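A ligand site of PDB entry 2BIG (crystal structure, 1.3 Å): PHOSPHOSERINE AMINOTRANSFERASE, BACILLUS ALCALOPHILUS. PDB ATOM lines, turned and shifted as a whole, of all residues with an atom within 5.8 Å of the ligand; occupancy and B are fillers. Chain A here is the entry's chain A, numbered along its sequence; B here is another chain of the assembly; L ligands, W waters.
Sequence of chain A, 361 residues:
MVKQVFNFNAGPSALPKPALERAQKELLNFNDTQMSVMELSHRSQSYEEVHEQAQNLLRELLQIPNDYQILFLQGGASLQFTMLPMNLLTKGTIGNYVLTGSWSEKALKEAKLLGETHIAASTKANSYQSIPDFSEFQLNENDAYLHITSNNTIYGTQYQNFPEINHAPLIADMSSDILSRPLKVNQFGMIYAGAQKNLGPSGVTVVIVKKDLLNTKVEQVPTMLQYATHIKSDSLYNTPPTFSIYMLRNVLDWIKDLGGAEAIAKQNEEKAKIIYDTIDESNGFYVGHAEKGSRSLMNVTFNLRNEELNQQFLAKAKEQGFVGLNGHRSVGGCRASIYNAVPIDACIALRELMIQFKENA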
ATOM      1  N   GLY A  75     -15.363  -3.141 -13.026  1.00  0.00           N
ATOM      2  CA  GLY A  75     -16.269  -3.611 -12.030  1.00  0.00           C
ATOM      3  C   GLY A  75     -16.517  -2.740 -10.830  1.00  0.00           C
ATOM      4  O   GLY A  75     -17.413  -2.990 -10.000  1.00  0.00           O
ATOM      5  N   GLY A  76     -15.684  -1.702 -10.690  1.00  0.00           N
ATOM      6  CA  GLY A  76     -15.816  -0.769  -9.575  1.00  0.00           C
ATOM      7  C   GLY A  76     -15.184  -1.316  -8.316  1.00  0.00           C
ATOM      8  O   GLY A  76     -14.757  -2.450  -8.214  1.00  0.00           O
ATOM      9  N   ALA A  77     -15.118  -0.451  -7.292  1.00  0.00           N
ATOM     10  CA  ALA A  77     -14.720  -0.940  -5.987  1.00  0.00           C
ATOM     11  C   ALA A  77     -15.674  -2.020  -5.525  1.00  0.00           C
ATOM     12  O   ALA A  77     -15.251  -2.927  -4.791  1.00  0.00           O
ATOM     13  CB  ALA A  77     -14.671   0.210  -4.984  1.00  0.00           C
ATOM     14  N   SER A  78     -16.936  -1.953  -5.949  1.00  0.00           N
ATOM     15  CA  SER A  78     -17.869  -2.963  -5.448  1.00  0.00           C
ATOM     16  C   SER A  78     -17.506  -4.358  -5.870  1.00  0.00           C
ATOM     17  O   SER A  78     -17.706  -5.301  -5.118  1.00  0.00           O
ATOM     18  CB  SER A  78     -19.290  -2.661  -5.954  1.00  0.00           C
ATOM     19  OG  SER A  78     -19.752  -1.420  -5.431  1.00  0.00           O
ATOM     20  N   LEU A  79     -16.912  -4.538  -7.071  1.00  0.00           N
ATOM     21  CA  LEU A  79     -16.447  -5.867  -7.425  1.00  0.00           C
ATOM     22  C   LEU A  79     -15.288  -6.297  -6.581  1.00  0.00           C
ATOM     23  O   LEU A  79     -15.149  -7.505  -6.259  1.00  0.00           O
ATOM     24  CB  LEU A  79     -16.128  -5.977  -8.939  1.00  0.00           C
ATOM     25  CG  LEU A  79     -15.890  -7.427  -9.405  1.00  0.00           C
ATOM     26  CD1 LEU A  79     -17.129  -8.300  -9.250  1.00  0.00           C
ATOM     27  CD2 LEU A  79     -15.450  -7.432 -10.832  1.00  0.00           C
ATOM     28  N   PHE A  81     -14.996  -5.771  -3.477  1.00  0.00           N
ATOM     29  CA  PHE A  81     -15.519  -6.267  -2.202  1.00  0.00           C
ATOM     30  C   PHE A  81     -15.645  -7.773  -2.234  1.00  0.00           C
ATOM     31  O   PHE A  81     -15.460  -8.419  -1.206  1.00  0.00           O
ATOM     32  CB  PHE A  81     -16.867  -5.673  -1.862  1.00  0.00           C
ATOM     33  CG  PHE A  81     -16.958  -4.166  -1.668  1.00  0.00           C
ATOM     34  CD1 PHE A  81     -18.167  -3.516  -1.751  1.00  0.00           C
ATOM     35  CD2 PHE A  81     -15.828  -3.414  -1.366  1.00  0.00           C
ATOM     36  CE1 PHE A  81     -18.316  -2.153  -1.523  1.00  0.00           C
ATOM     37  CE2 PHE A  81     -15.952  -2.053  -1.121  1.00  0.00           C
ATOM     38  CZ  PHE A  81     -17.155  -1.467  -1.186  1.00  0.00           C
ATOM     39  N   TRP A 103     -19.652   2.165   3.420  1.00  0.00           N
ATOM     40  CA  TRP A 103     -18.828   1.408   2.484  1.00  0.00           C
ATOM     41  C   TRP A 103     -18.070   0.281   3.144  1.00  0.00           C
ATOM     42  O   TRP A 103     -17.870  -0.800   2.582  1.00  0.00           O
ATOM     43  CB  TRP A 103     -17.890   2.366   1.707  1.00  0.00           C
ATOM     44  CG  TRP A 103     -18.698   3.210   0.734  1.00  0.00           C
ATOM     45  CD1 TRP A 103     -18.826   4.556   0.747  1.00  0.00           C
ATOM     46  CD2 TRP A 103     -19.463   2.748  -0.361  1.00  0.00           C
ATOM     47  NE1 TRP A 103     -19.637   4.973  -0.289  1.00  0.00           N
ATOM     48  CE2 TRP A 103     -20.032   3.869  -0.988  1.00  0.00           C
ATOM     49  CE3 TRP A 103     -19.709   1.461  -0.885  1.00  0.00           C
ATOM     50  CZ2 TRP A 103     -20.837   3.780  -2.098  1.00  0.00           C
ATOM     51  CZ3 TRP A 103     -20.510   1.362  -1.996  1.00  0.00           C
ATOM     52  CH2 TRP A 103     -21.062   2.509  -2.584  1.00  0.00           C
ATOM     53  N   THR A 149     -11.376   1.171   5.382  1.00  0.00           N
ATOM     54  CA  THR A 149     -11.903   2.122   4.401  1.00  0.00           C
ATOM     55  C   THR A 149     -11.253   3.435   4.787  1.00  0.00           C
ATOM     56  O   THR A 149     -11.589   4.029   5.810  1.00  0.00           O
ATOM     57  CB  THR A 149     -13.413   2.223   4.498  1.00  0.00           C
ATOM     58  OG1 THR A 149     -13.979   0.902   4.474  1.00  0.00           O
ATOM     59  CG2 THR A 149     -13.959   3.044   3.315  1.00  0.00           C
ATOM     60  N   ASN A 151     -11.267   6.573   3.628  1.00  0.00           N
ATOM     61  CA  ASN A 151     -12.129   7.738   3.610  1.00  0.00           C
ATOM     62  C   ASN A 151     -13.562   7.232   3.468  1.00  0.00           C
ATOM     63  O   ASN A 151     -13.930   6.533   2.543  1.00  0.00           O
ATOM     64  CB  ASN A 151     -11.743   8.717   2.489  1.00  0.00           C
ATOM     65  CG  ASN A 151     -12.513  10.024   2.603  1.00  0.00           C
ATOM     66  OD1 ASN A 151     -12.104  10.864   3.445  1.00  0.00           O
ATOM     67  ND2 ASN A 151     -13.570  10.165   1.828  1.00  0.00           N
ATOM     68  N   ASN A 152     -14.364   7.551   4.491  1.00  0.00           N
ATOM     69  CA  ASN A 152     -15.725   7.054   4.592  1.00  0.00           C
ATOM     70  C   ASN A 152     -16.631   8.091   3.940  1.00  0.00           C
ATOM     71  O   ASN A 152     -17.091   9.034   4.576  1.00  0.00           O
ATOM     72  CB  ASN A 152     -16.070   6.772   6.049  1.00  0.00           C
ATOM     73  CG  ASN A 152     -15.039   5.831   6.624  1.00  0.00           C
ATOM     74  OD1 ASN A 152     -15.098   4.627   6.359  1.00  0.00           O
ATOM     75  ND2 ASN A 152     -14.097   6.375   7.413  1.00  0.00           N
ATOM     76  N   THR A 153     -16.843   7.881   2.621  1.00  0.00           N
ATOM     77  CA  THR A 153     -17.378   8.886   1.733  1.00  0.00           C
ATOM     78  C   THR A 153     -18.727   9.416   2.203  1.00  0.00           C
ATOM     79  O   THR A 153     -19.057  10.587   1.968  1.00  0.00           O
ATOM     80  CB  THR A 153     -17.539   8.240   0.325  1.00  0.00           C
ATOM     81  OG1 THR A 153     -16.428   7.338   0.142  1.00  0.00           O
ATOM     82  CG2 THR A 153     -17.553   9.280  -0.778  1.00  0.00           C
ATOM     83  N   ASP A 173      -9.778   0.064   1.011  1.00  0.00           N
ATOM     84  CA  ASP A 173     -10.653   0.729   0.063  1.00  0.00           C
ATOM     85  C   ASP A 173     -10.356   2.232   0.150  1.00  0.00           C
ATOM     86  O   ASP A 173     -10.805   2.873   1.110  1.00  0.00           O
ATOM     87  CB  ASP A 173     -12.125   0.428   0.397  1.00  0.00           C
ATOM     88  CG  ASP A 173     -13.072   1.149  -0.520  1.00  0.00           C
ATOM     89  OD1 ASP A 173     -12.639   1.915  -1.431  1.00  0.00           O
ATOM     90  OD2 ASP A 173     -14.295   0.943  -0.310  1.00  0.00           O
ATOM     91  N   MET A 174      -9.585   2.732  -0.796  1.00  0.00           N
ATOM     92  CA  MET A 174      -9.187   4.124  -0.847  1.00  0.00           C
ATOM     93  C   MET A 174      -9.925   4.886  -1.944  1.00  0.00           C
ATOM     94  O   MET A 174      -9.417   5.913  -2.415  1.00  0.00           O
ATOM     95  CB  MET A 174      -7.702   4.278  -1.035  1.00  0.00           C
ATOM     96  CG  MET A 174      -6.904   3.631   0.117  1.00  0.00           C
ATOM     97  SD  MET A 174      -5.199   4.158   0.089  1.00  0.00           S
ATOM     98  CE  MET A 174      -4.550   3.458   1.594  1.00  0.00           C
ATOM     99  N   SER A 175     -11.082   4.389  -2.347  1.00  0.00           N
ATOM    100  CA  SER A 175     -11.822   4.990  -3.448  1.00  0.00           C
ATOM    101  C   SER A 175     -11.933   6.517  -3.342  1.00  0.00           C
ATOM    102  O   SER A 175     -11.699   7.181  -4.338  1.00  0.00           O
ATOM    103  CB  SER A 175     -13.232   4.445  -3.524  1.00  0.00           C
ATOM    104  OG  SER A 175     -13.220   3.046  -3.834  1.00  0.00           O
ATOM    105  N   SER A 176     -12.242   7.066  -2.162  1.00  0.00           N
ATOM    106  CA  SER A 176     -12.548   8.492  -2.121  1.00  0.00           C
ATOM    107  C   SER A 176     -11.385   9.337  -1.619  1.00  0.00           C
ATOM    108  O   SER A 176     -11.580  10.539  -1.479  1.00  0.00           O
ATOM    109  CB  SER A 176     -13.877   8.729  -1.389  1.00  0.00           C
ATOM    110  OG  SER A 176     -13.840   8.103  -0.117  1.00  0.00           O
ATOM    111  N   GLY A 194     -12.095   2.755  -6.984  1.00  0.00           N
ATOM    112  CA  GLY A 194     -12.742   3.187  -8.214  1.00  0.00           C
ATOM    113  C   GLY A 194     -12.151   4.488  -8.629  1.00  0.00           C
ATOM    114  O   GLY A 194     -11.886   5.369  -7.775  1.00  0.00           O
ATOM    115  N   GLN A 196     -13.395   7.055 -10.142  1.00  0.00           N
ATOM    116  CA  GLN A 196     -14.300   8.159 -10.418  1.00  0.00           C
ATOM    117  C   GLN A 196     -14.438   9.164  -9.291  1.00  0.00           C
ATOM    118  O   GLN A 196     -15.264  10.056  -9.362  1.00  0.00           O
ATOM    119  CB  GLN A 196     -15.660   7.623 -10.753  1.00  0.00           C
ATOM    120  CG  GLN A 196     -16.388   6.909  -9.626  1.00  0.00           C
ATOM    121  CD  GLN A 196     -16.144   5.407  -9.549  1.00  0.00           C
ATOM    122  OE1 GLN A 196     -15.222   4.879 -10.210  1.00  0.00           O
ATOM    123  NE2 GLN A 196     -16.950   4.709  -8.724  1.00  0.00           N
ATOM    124  N   LYS A 197     -13.701   9.045  -8.177  1.00  0.00           N
ATOM    125  CA  LYS A 197     -13.775  10.140  -7.198  1.00  0.00           C
ATOM    126  C   LYS A 197     -12.591  11.077  -7.333  1.00  0.00           C
ATOM    127  O   LYS A 197     -12.719  12.294  -7.455  1.00  0.00           O
ATOM    128  CB  LYS A 197     -13.999   9.649  -5.774  1.00  0.00           C
ATOM    129  CG  LYS A 197     -14.364   8.246  -5.425  1.00  0.00           C
ATOM    130  CD  LYS A 197     -15.814   7.855  -5.601  1.00  0.00           C
ATOM    131  CE  LYS A 197     -16.541   7.477  -4.365  1.00  0.00           C
ATOM    132  NZ  LYS A 197     -17.402   6.252  -4.456  1.00  0.00           N
ATOM    133  N   THR A 205     -11.054   0.651 -12.150  1.00  0.00           N
ATOM    134  CA  THR A 205     -10.715   0.516 -10.737  1.00  0.00           C
ATOM    135  C   THR A 205      -9.226   0.276 -10.673  1.00  0.00           C
ATOM    136  O   THR A 205      -8.702  -0.628 -11.358  1.00  0.00           O
ATOM    137  CB  THR A 205     -11.497  -0.649 -10.130  1.00  0.00           C
ATOM    138  OG1 THR A 205     -12.900  -0.380 -10.275  1.00  0.00           O
ATOM    139  CG2 THR A 205     -11.246  -0.844  -8.655  1.00  0.00           C
ATOM    140  N   TYR A 339     -12.897  16.680  -3.707  1.00  0.00           N
ATOM    141  CA  TYR A 339     -11.817  15.879  -4.226  1.00  0.00           C
ATOM    142  C   TYR A 339     -10.758  16.758  -4.900  1.00  0.00           C
ATOM    143  O   TYR A 339     -10.972  17.980  -5.091  1.00  0.00           O
ATOM    144  CB  TYR A 339     -12.459  14.933  -5.260  1.00  0.00           C
ATOM    145  CG  TYR A 339     -13.501  14.019  -4.731  1.00  0.00           C
ATOM    146  CD1 TYR A 339     -14.752  13.928  -5.282  1.00  0.00           C
ATOM    147  CD2 TYR A 339     -13.210  13.182  -3.632  1.00  0.00           C
ATOM    148  CE1 TYR A 339     -15.726  13.089  -4.831  1.00  0.00           C
ATOM    149  CE2 TYR A 339     -14.200  12.358  -3.178  1.00  0.00           C
ATOM    150  CZ  TYR A 339     -15.442  12.294  -3.750  1.00  0.00           C
ATOM    151  OH  TYR A 339     -16.391  11.415  -3.223  1.00  0.00           O
ATOM    152  N   HIS B  42     -23.892   9.604 -11.170  1.00  0.00           N
ATOM    153  CA  HIS B  42     -24.745   8.633 -11.831  1.00  0.00           C
ATOM    154  C   HIS B  42     -26.134   8.577 -11.199  1.00  0.00           C
ATOM    155  O   HIS B  42     -27.002   7.902 -11.749  1.00  0.00           O
ATOM    156  CB  HIS B  42     -24.189   7.201 -11.806  1.00  0.00           C
ATOM    157  CG  HIS B  42     -24.021   6.669 -10.409  1.00  0.00           C
ATOM    158  ND1 HIS B  42     -23.191   7.298  -9.471  1.00  0.00           N
ATOM    159  CD2 HIS B  42     -24.600   5.633  -9.767  1.00  0.00           C
ATOM    160  CE1 HIS B  42     -23.261   6.621  -8.336  1.00  0.00           C
ATOM    161  NE2 HIS B  42     -24.103   5.601  -8.485  1.00  0.00           N
ATOM    162  N   GLN B  74     -20.164  -3.948 -16.342  1.00  0.00           N
ATOM    163  CA  GLN B  74     -18.719  -3.925 -16.568  1.00  0.00           C
ATOM    164  C   GLN B  74     -18.194  -5.348 -16.670  1.00  0.00           C
ATOM    165  O   GLN B  74     -18.832  -6.312 -16.261  1.00  0.00           O
ATOM    166  CB  GLN B  74     -18.038  -3.186 -15.444  1.00  0.00           C
ATOM    167  CG  GLN B  74     -18.530  -1.721 -15.295  1.00  0.00           C
ATOM    168  CD  GLN B  74     -17.730  -1.029 -14.229  1.00  0.00           C
ATOM    169  OE1 GLN B  74     -16.488  -0.889 -14.333  1.00  0.00           O
ATOM    170  NE2 GLN B  74     -18.424  -0.586 -13.168  1.00  0.00           N
ATOM    171  N   ASN B 238     -24.176  -0.132  -8.584  1.00  0.00           N
ATOM    172  CA  ASN B 238     -22.949   0.616  -8.295  1.00  0.00           C
ATOM    173  C   ASN B 238     -22.741   1.595  -9.452  1.00  0.00           C
ATOM    174  O   ASN B 238     -23.611   1.751 -10.323  1.00  0.00           O
ATOM    175  CB  ASN B 238     -21.741  -0.274  -8.037  1.00  0.00           C
ATOM    176  CG  ASN B 238     -21.180  -0.936  -9.276  1.00  0.00           C
ATOM    177  OD1 ASN B 238     -21.928  -1.298 -10.199  1.00  0.00           O
ATOM    178  ND2 ASN B 238     -19.846  -1.102  -9.269  1.00  0.00           N
ATOM    179  N   THR B 239     -21.599   2.268  -9.456  1.00  0.00           N
ATOM    180  CA  THR B 239     -21.385   3.312 -10.460  1.00  0.00           C
ATOM    181  C   THR B 239     -21.195   2.669 -11.828  1.00  0.00           C
ATOM    182  O   THR B 239     -20.285   1.862 -12.019  1.00  0.00           O
ATOM    183  CB  THR B 239     -20.155   4.153 -10.119  1.00  0.00           C
ATOM    184  OG1 THR B 239     -20.211   4.590  -8.755  1.00  0.00           O
ATOM    185  CG2 THR B 239     -20.090   5.367 -11.006  1.00  0.00           C
HETATM  186  N1  LIG L   1     -16.051   2.473  -1.655  1.00  0.00           N
HETATM  187  C1  LIG L   1     -16.020   3.806  -1.383  1.00  0.00           C
HETATM  188  C2  LIG L   1     -15.189   4.296  -0.195  1.00  0.00           C
HETATM  189  C3  LIG L   1     -16.688   4.670  -2.224  1.00  0.00           C
HETATM  190  O1  LIG L   1     -16.648   5.989  -2.004  1.00  0.00           O
HETATM  191  C4  LIG L   1     -17.411   4.182  -3.326  1.00  0.00           C
HETATM  192  C5  LIG L   1     -18.283   5.048  -4.220  1.00  0.00           C
HETATM  193  C6  LIG L   1     -17.470   2.802  -3.536  1.00  0.00           C
HETATM  194  C7  LIG L   1     -16.786   1.962  -2.665  1.00  0.00           C
HETATM  195  C8  LIG L   1     -18.312   2.149  -4.635  1.00  0.00           C
HETATM  196  O2  LIG L   1     -17.587   2.249  -5.888  1.00  0.00           O
HETATM  197  P1  LIG L   1     -18.245   1.646  -7.254  1.00  0.00           P
HETATM  198  O3  LIG L   1     -19.511   2.378  -7.438  1.00  0.00           O
HETATM  199  O4  LIG L   1     -18.443   0.174  -6.992  1.00  0.00           O
HETATM  200  O5  LIG L   1     -17.184   1.909  -8.268  1.00  0.00           O
HETATM  201  O   HOH W   1     -15.054   3.467  -6.037  1.00  0.00           O
HETATM  202  O   HOH W   2     -20.859   6.289  -5.344  1.00  0.00           O
HETATM  203  O   HOH W   3     -21.727   2.739  -5.929  1.00  0.00           O
HETATM  204  O   HOH W   4     -17.832   1.370 -10.908  1.00  0.00           O
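NZ of Lys 197 is covalently linked to C5 of the ligand (1.5 Å). OG1 of Thr 153 lies within hydrogen-bond range of O1 of the ligand. The backbone NH of Ser 78 lies within hydrogen-bond range of an oxygen (O4) of the ligand (2.8 Å). OG of Ser 78 lies within hydrogen-bond range of O4 of the ligand (2.6 Å). O3 of the ligand lies within hydrogen-bond range of N of Thr 239 of chain B (2.9 Å). O3 of the ligand sits at hydrogen-bond distance from OG1 of Thr 239 of chain B. OD2 of Asp 173 lies within hydrogen-bond range of N1 of the ligand, at 2.7 Å. The side-chain amide nitrogen (NE2) of Gln 196 sits at hydrogen-bond distance from an oxygen (O5) of the ligand (2.8 Å). An oxygen (O4) of the ligand lies within hydrogen-bond range of the side-chain amide nitrogen of Asn 238 of chain B (3.0 Å). N of Ala 77 is in hydrogen-bond range of O5 of the ligand (3.3 Å).
Water W4 lies within hydrogen-bond range of the backbone carbonyl oxygen of Thr 239 of chain B (2.7 Å), an oxygen (O5) of the ligand (2.8 Å) and the side-chain amide nitrogen of Gln 74 of chain B (3.0 Å). Water W1 lies within hydrogen-bond range of an oxygen (O2) of the ligand, the side-chain hydroxyl of Ser 175 and the backbone NH of Gly 194.
Residues that only touch the ligand: Gly 76, Trp 103, Ser 175, Phe 81, Asn 151, Thr 149 and Ser 176. Hydrophobic or aromatic side chains that line the ligand: Ala 77, Phe 81 and Trp 103. 15 residues have an atom within 4 Å of the ligand: Gly 76, Ala 77, Ser 78, Phe 81, Trp 103, Thr 149, Asn 151, Thr 153, Asp 173, Ser 175, Ser 176, Gln 196, Lys 197, Asn 238 of chain B and Thr 239 of chain B. The nearest printed residue that does not touch the ligand is Gly 75 (4.5 Å).
OG of Ser 176 sits at hydrogen-bond distance from OG1 of Thr 153 (2.7 Å). The side-chain hydroxyl (OG1) of Thr 239 of chain B sits at hydrogen-bond distance from the side-chain amide nitrogen (NE2) of Gln 196 (3.3 Å). The side-chain amide nitrogen (NE2) of Gln 74 of chain B sits at hydrogen-bond distance from the backbone carbonyl oxygen (O) of Thr 239 of chain B, 3.3 Å away. The side-chain carboxylate (OD1) of Asp 173 is in hydrogen-bond range of the side-chain hydroxyl (OG) of Ser 175, 2.7 Å away. ND2 of Asn 238 of chain B lies within hydrogen-bond range of O of Gly 75, at 3.2 Å. The backbone NH (N) of Gly 76 sits close to the side-chain hydroxyl (OG1) of Thr 205, 3.1 Å away. N of Gly 194 lies within hydrogen-bond range of OG of Ser 175 (3.4 Å). ND2 of Asn 151 is in hydrogen-bond range of OG of Ser 176, 2.8 Å away.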
